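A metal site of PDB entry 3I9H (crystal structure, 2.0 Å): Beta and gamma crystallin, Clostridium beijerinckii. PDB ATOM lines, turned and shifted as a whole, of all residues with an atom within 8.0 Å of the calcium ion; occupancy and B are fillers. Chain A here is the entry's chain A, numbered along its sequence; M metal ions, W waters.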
ATOM      1  N   LEU A  26      31.429 -19.792   4.646  1.00  0.00           N
ATOM      2  CA  LEU A  26      31.330 -21.244   4.560  1.00  0.00           C
ATOM      3  C   LEU A  26      32.663 -21.906   4.194  1.00  0.00           C
ATOM      4  O   LEU A  26      33.111 -22.828   4.874  1.00  0.00           O
ATOM      5  CB  LEU A  26      30.277 -21.641   3.526  1.00  0.00           C
ATOM      6  CG  LEU A  26      30.153 -23.152   3.268  1.00  0.00           C
ATOM      7  CD1 LEU A  26      29.699 -23.861   4.536  1.00  0.00           C
ATOM      8  CD2 LEU A  26      29.182 -23.396   2.137  1.00  0.00           C
ATOM      9  N   ASN A  36      29.273 -27.681   6.726  1.00  0.00           N
ATOM     10  CA  ASN A  36      28.045 -26.906   6.620  1.00  0.00           C
ATOM     11  C   ASN A  36      26.936 -27.635   7.399  1.00  0.00           C
ATOM     12  O   ASN A  36      26.990 -28.852   7.563  1.00  0.00           O
ATOM     13  CB  ASN A  36      27.649 -26.789   5.137  1.00  0.00           C
ATOM     14  CG  ASN A  36      26.692 -25.642   4.883  1.00  0.00           C
ATOM     15  OD1 ASN A  36      26.330 -24.912   5.799  1.00  0.00           O
ATOM     16  ND2 ASN A  36      26.284 -25.485   3.622  1.00  0.00           N
ATOM     17  N   ASP A  37      25.952 -26.869   7.876  1.00  0.00           N
ATOM     18  CA  ASP A  37      24.799 -27.423   8.609  1.00  0.00           C
ATOM     19  C   ASP A  37      25.209 -28.567   9.520  1.00  0.00           C
ATOM     20  O   ASP A  37      24.745 -29.700   9.373  1.00  0.00           O
ATOM     21  CB  ASP A  37      23.759 -27.889   7.602  1.00  0.00           C
ATOM     22  CG  ASP A  37      23.445 -26.831   6.573  1.00  0.00           C
ATOM     23  OD1 ASP A  37      23.396 -25.660   6.988  1.00  0.00           O
ATOM     24  OD2 ASP A  37      23.263 -27.142   5.377  1.00  0.00           O
ATOM     25  N   TRP A  38      26.040 -28.243  10.501  1.00  0.00           N
ATOM     26  CA  TRP A  38      26.600 -29.231  11.416  1.00  0.00           C
ATOM     27  C   TRP A  38      26.648 -28.801  12.886  1.00  0.00           C
ATOM     28  O   TRP A  38      26.712 -29.636  13.774  1.00  0.00           O
ATOM     29  CB  TRP A  38      28.006 -29.534  10.887  1.00  0.00           C
ATOM     30  CG  TRP A  38      28.993 -30.149  11.822  1.00  0.00           C
ATOM     31  CD1 TRP A  38      29.390 -31.462  11.847  1.00  0.00           C
ATOM     32  CD2 TRP A  38      29.812 -29.463  12.777  1.00  0.00           C
ATOM     33  NE1 TRP A  38      30.407 -31.625  12.748  1.00  0.00           N
ATOM     34  CE2 TRP A  38      30.690 -30.419  13.337  1.00  0.00           C
ATOM     35  CE3 TRP A  38      29.880 -28.137  13.223  1.00  0.00           C
ATOM     36  CZ2 TRP A  38      31.643 -30.095  14.317  1.00  0.00           C
ATOM     37  CZ3 TRP A  38      30.832 -27.801  14.191  1.00  0.00           C
ATOM     38  CH2 TRP A  38      31.697 -28.781  14.725  1.00  0.00           C
ATOM     39  N   TYR A  53      24.730 -17.478  11.141  1.00  0.00           N
ATOM     40  CA  TYR A  53      23.871 -17.252   9.990  1.00  0.00           C
ATOM     41  C   TYR A  53      23.439 -18.520   9.262  1.00  0.00           C
ATOM     42  O   TYR A  53      24.218 -19.456   9.068  1.00  0.00           O
ATOM     43  CB  TYR A  53      24.552 -16.310   8.990  1.00  0.00           C
ATOM     44  CG  TYR A  53      24.794 -14.926   9.551  1.00  0.00           C
ATOM     45  CD1 TYR A  53      25.843 -14.690  10.455  1.00  0.00           C
ATOM     46  CD2 TYR A  53      23.979 -13.853   9.190  1.00  0.00           C
ATOM     47  CE1 TYR A  53      26.064 -13.404  10.982  1.00  0.00           C
ATOM     48  CE2 TYR A  53      24.198 -12.582   9.709  1.00  0.00           C
ATOM     49  CZ  TYR A  53      25.231 -12.360  10.607  1.00  0.00           C
ATOM     50  OH  TYR A  53      25.434 -11.103  11.121  1.00  0.00           O
ATOM     51  N   GLU A  54      22.177 -18.512   8.833  1.00  0.00           N
ATOM     52  CA  GLU A  54      21.599 -19.628   8.110  1.00  0.00           C
ATOM     53  C   GLU A  54      22.296 -19.807   6.775  1.00  0.00           C
ATOM     54  O   GLU A  54      22.559 -20.924   6.367  1.00  0.00           O
ATOM     55  CB  GLU A  54      20.106 -19.388   7.864  1.00  0.00           C
ATOM     56  CG  GLU A  54      19.448 -20.478   7.038  1.00  0.00           C
ATOM     57  CD  GLU A  54      18.066 -20.070   6.557  1.00  0.00           C
ATOM     58  OE1 GLU A  54      17.411 -20.883   5.877  1.00  0.00           O
ATOM     59  OE2 GLU A  54      17.642 -18.932   6.846  1.00  0.00           O
ATOM     60  N   ASN A  55      22.607 -18.728   6.086  1.00  0.00           N
ATOM     61  CA  ASN A  55      23.257 -18.856   4.794  1.00  0.00           C
ATOM     62  C   ASN A  55      24.680 -18.330   4.765  1.00  0.00           C
ATOM     63  O   ASN A  55      25.176 -17.794   5.754  1.00  0.00           O
ATOM     64  CB  ASN A  55      22.410 -18.170   3.712  1.00  0.00           C
ATOM     65  CG  ASN A  55      21.015 -18.748   3.630  1.00  0.00           C
ATOM     66  OD1 ASN A  55      20.830 -19.960   3.742  1.00  0.00           O
ATOM     67  ND2 ASN A  55      20.019 -17.888   3.411  1.00  0.00           N
ATOM     68  N   ASP A  56      25.336 -18.508   3.621  1.00  0.00           N
ATOM     69  CA  ASP A  56      26.711 -18.062   3.468  1.00  0.00           C
ATOM     70  C   ASP A  56      26.801 -16.550   3.425  1.00  0.00           C
ATOM     71  O   ASP A  56      25.814 -15.853   3.164  1.00  0.00           O
ATOM     72  CB  ASP A  56      27.321 -18.650   2.193  1.00  0.00           C
ATOM     73  CG  ASP A  56      28.841 -18.638   2.216  1.00  0.00           C
ATOM     74  OD1 ASP A  56      29.414 -18.141   3.207  1.00  0.00           O
ATOM     75  OD2 ASP A  56      29.464 -19.126   1.242  1.00  0.00           O
ATOM     76  N   THR A  59      24.220 -13.995   5.688  1.00  0.00           N
ATOM     77  CA  THR A  59      22.873 -13.663   5.241  1.00  0.00           C
ATOM     78  C   THR A  59      21.950 -14.781   5.672  1.00  0.00           C
ATOM     79  O   THR A  59      22.388 -15.802   6.204  1.00  0.00           O
ATOM     80  CB  THR A  59      22.804 -13.471   3.702  1.00  0.00           C
ATOM     81  OG1 THR A  59      23.348 -14.618   3.045  1.00  0.00           O
ATOM     82  CG2 THR A  59      23.569 -12.213   3.290  1.00  0.00           C
ATOM     83  N   TRP A  63      21.044 -16.062  14.269  1.00  0.00           N
ATOM     84  CA  TRP A  63      20.825 -16.475  15.652  1.00  0.00           C
ATOM     85  C   TRP A  63      22.007 -15.935  16.430  1.00  0.00           C
ATOM     86  O   TRP A  63      23.149 -16.006  15.977  1.00  0.00           O
ATOM     87  CB  TRP A  63      20.767 -18.001  15.763  1.00  0.00           C
ATOM     88  CG  TRP A  63      19.548 -18.630  15.146  1.00  0.00           C
ATOM     89  CD1 TRP A  63      18.300 -18.720  15.691  1.00  0.00           C
ATOM     90  CD2 TRP A  63      19.477 -19.268  13.862  1.00  0.00           C
ATOM     91  NE1 TRP A  63      17.455 -19.376  14.829  1.00  0.00           N
ATOM     92  CE2 TRP A  63      18.150 -19.732  13.702  1.00  0.00           C
ATOM     93  CE3 TRP A  63      20.405 -19.502  12.833  1.00  0.00           C
ATOM     94  CZ2 TRP A  63      17.723 -20.404  12.545  1.00  0.00           C
ATOM     95  CZ3 TRP A  63      19.980 -20.172  11.685  1.00  0.00           C
ATOM     96  CH2 TRP A  63      18.653 -20.611  11.553  1.00  0.00           C
ATOM     97  N   ALA A  76      17.553 -23.582  15.067  1.00  0.00           N
ATOM     98  CA  ALA A  76      18.890 -23.217  14.634  1.00  0.00           C
ATOM     99  C   ALA A  76      19.812 -24.413  14.379  1.00  0.00           C
ATOM    100  O   ALA A  76      20.873 -24.273  13.768  1.00  0.00           O
ATOM    101  CB  ALA A  76      19.538 -22.284  15.656  1.00  0.00           C
ATOM    102  N   ASN A  77      19.413 -25.591  14.840  1.00  0.00           N
ATOM    103  CA  ASN A  77      20.242 -26.777  14.672  1.00  0.00           C
ATOM    104  C   ASN A  77      20.612 -27.119  13.220  1.00  0.00           C
ATOM    105  O   ASN A  77      19.790 -27.039  12.318  1.00  0.00           O
ATOM    106  CB  ASN A  77      19.587 -28.009  15.307  1.00  0.00           C
ATOM    107  CG  ASN A  77      20.528 -29.193  15.344  1.00  0.00           C
ATOM    108  OD1 ASN A  77      21.631 -29.103  15.899  1.00  0.00           O
ATOM    109  ND2 ASN A  77      20.113 -30.302  14.735  1.00  0.00           N
ATOM    110  N   ASP A  78      21.866 -27.522  13.038  1.00  0.00           N
ATOM    111  CA  ASP A  78      22.386 -27.895  11.729  1.00  0.00           C
ATOM    112  C   ASP A  78      22.073 -26.890  10.635  1.00  0.00           C
ATOM    113  O   ASP A  78      21.723 -27.282   9.510  1.00  0.00           O
ATOM    114  CB  ASP A  78      21.848 -29.275  11.330  1.00  0.00           C
ATOM    115  CG  ASP A  78      22.405 -30.383  12.201  1.00  0.00           C
ATOM    116  OD1 ASP A  78      23.372 -30.082  12.926  1.00  0.00           O
ATOM    117  OD2 ASP A  78      21.903 -31.536  12.145  1.00  0.00           O
ATOM    118  N   LYS A  79      22.208 -25.609  10.942  1.00  0.00           N
ATOM    119  CA  LYS A  79      21.941 -24.577   9.950  1.00  0.00           C
ATOM    120  C   LYS A  79      23.094 -23.607   9.724  1.00  0.00           C
ATOM    121  O   LYS A  79      23.114 -22.883   8.744  1.00  0.00           O
ATOM    122  CB  LYS A  79      20.673 -23.819  10.313  1.00  0.00           C
ATOM    123  CG  LYS A  79      19.455 -24.711  10.458  1.00  0.00           C
ATOM    124  CD  LYS A  79      18.161 -23.927  10.341  1.00  0.00           C
ATOM    125  CE  LYS A  79      17.970 -23.380   8.939  1.00  0.00           C
ATOM    126  NZ  LYS A  79      16.656 -22.666   8.774  1.00  0.00           N
ATOM    127  N   MET A  80      24.069 -23.581  10.627  1.00  0.00           N
ATOM    128  CA  MET A  80      25.177 -22.651  10.455  1.00  0.00           C
ATOM    129  C   MET A  80      25.956 -22.852   9.151  1.00  0.00           C
ATOM    130  O   MET A  80      26.428 -23.949   8.868  1.00  0.00           O
ATOM    131  CB  MET A  80      26.144 -22.756  11.644  1.00  0.00           C
ATOM    132  CG  MET A  80      27.257 -21.718  11.579  1.00  0.00           C
ATOM    133  SD  MET A  80      28.274 -21.652  13.084  1.00  0.00           S
ATOM    134  CE  MET A  80      29.423 -23.006  12.760  1.00  0.00           C
ATOM    135  N   THR A  81      26.072 -21.768   8.372  1.00  0.00           N
ATOM    136  CA  THR A  81      26.794 -21.768   7.101  1.00  0.00           C
ATOM    137  C   THR A  81      27.873 -20.680   7.118  1.00  0.00           C
ATOM    138  O   THR A  81      28.861 -20.761   6.385  1.00  0.00           O
ATOM    139  CB  THR A  81      25.850 -21.549   5.914  1.00  0.00           C
ATOM    140  OG1 THR A  81      25.067 -22.734   5.736  1.00  0.00           O
ATOM    141  CG2 THR A  81      26.616 -21.297   4.623  1.00  0.00           C
ATOM    142  N   SER A  82      27.662 -19.657   7.939  1.00  0.00           N
ATOM    143  CA  SER A  82      28.631 -18.576   8.119  1.00  0.00           C
ATOM    144  C   SER A  82      28.404 -18.068   9.533  1.00  0.00           C
ATOM    145  O   SER A  82      27.339 -18.277  10.113  1.00  0.00           O
ATOM    146  CB  SER A  82      28.443 -17.448   7.079  1.00  0.00           C
ATOM    147  OG  SER A  82      27.186 -16.821   7.181  1.00  0.00           O
HETATM  148 CA    CA M   1      22.648 -23.419   6.214  1.00  0.00          CA
HETATM  149  O   HOH W   1      21.561 -22.483   3.840  1.00  0.00           O
HETATM  150  O   HOH W   2      22.919 -24.734   3.774  1.00  0.00           O
HETATM  151  O   HOH W   3      20.300 -24.298   6.869  1.00  0.00           O
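Merely in contact with the calcium ion: Asn 36.
Five residues have an atom within 4 Å of the calcium ion: Asn 36, Asp 37, Glu 54, Lys 79 and Thr 81.
The backbone NH (N) of Leu 26 sits close to the backbone carbonyl oxygen (O) of Thr 81.
N of Thr 81 is in hydrogen-bond range of O of Tyr 53 (3.0 Å).
The side-chain hydroxyl of Thr 81 lies close to the side-chain amide oxygen of Asn 36 (2.5 Å).
The backbone NH of Asp 37 sits at hydrogen-bond distance from the backbone carbonyl oxygen of Met 80 (3.1 Å).
The side-chain amide oxygen of Asn 36 lies close to the backbone carbonyl oxygen of Met 80 (3.2 Å).
OD1 of Asp 37 sits close to OD1 of Asn 36.
Water W2 bridges the side-chain carboxylate of Asp 37 (2.9 Å) and the side-chain amide nitrogen of Asn 36 (3.5 Å).
OD1 of Asp 37 binds the calcium ion (2.5 Å).
O of Glu 54 is bound to the calcium ion (2.5 Å).
OG1 of Thr 81 binds the calcium ion, at 2.6 Å.
Water W3 is bound to the calcium ion.
O of Lys 79 is bound to the calcium ion (2.6 Å).
Water W1 is bound to the calcium ion, at 2.8 Å.
The calcium ion is bound by water W2 (2.8 Å).
The calcium ion has seven donor atoms within binding distance.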
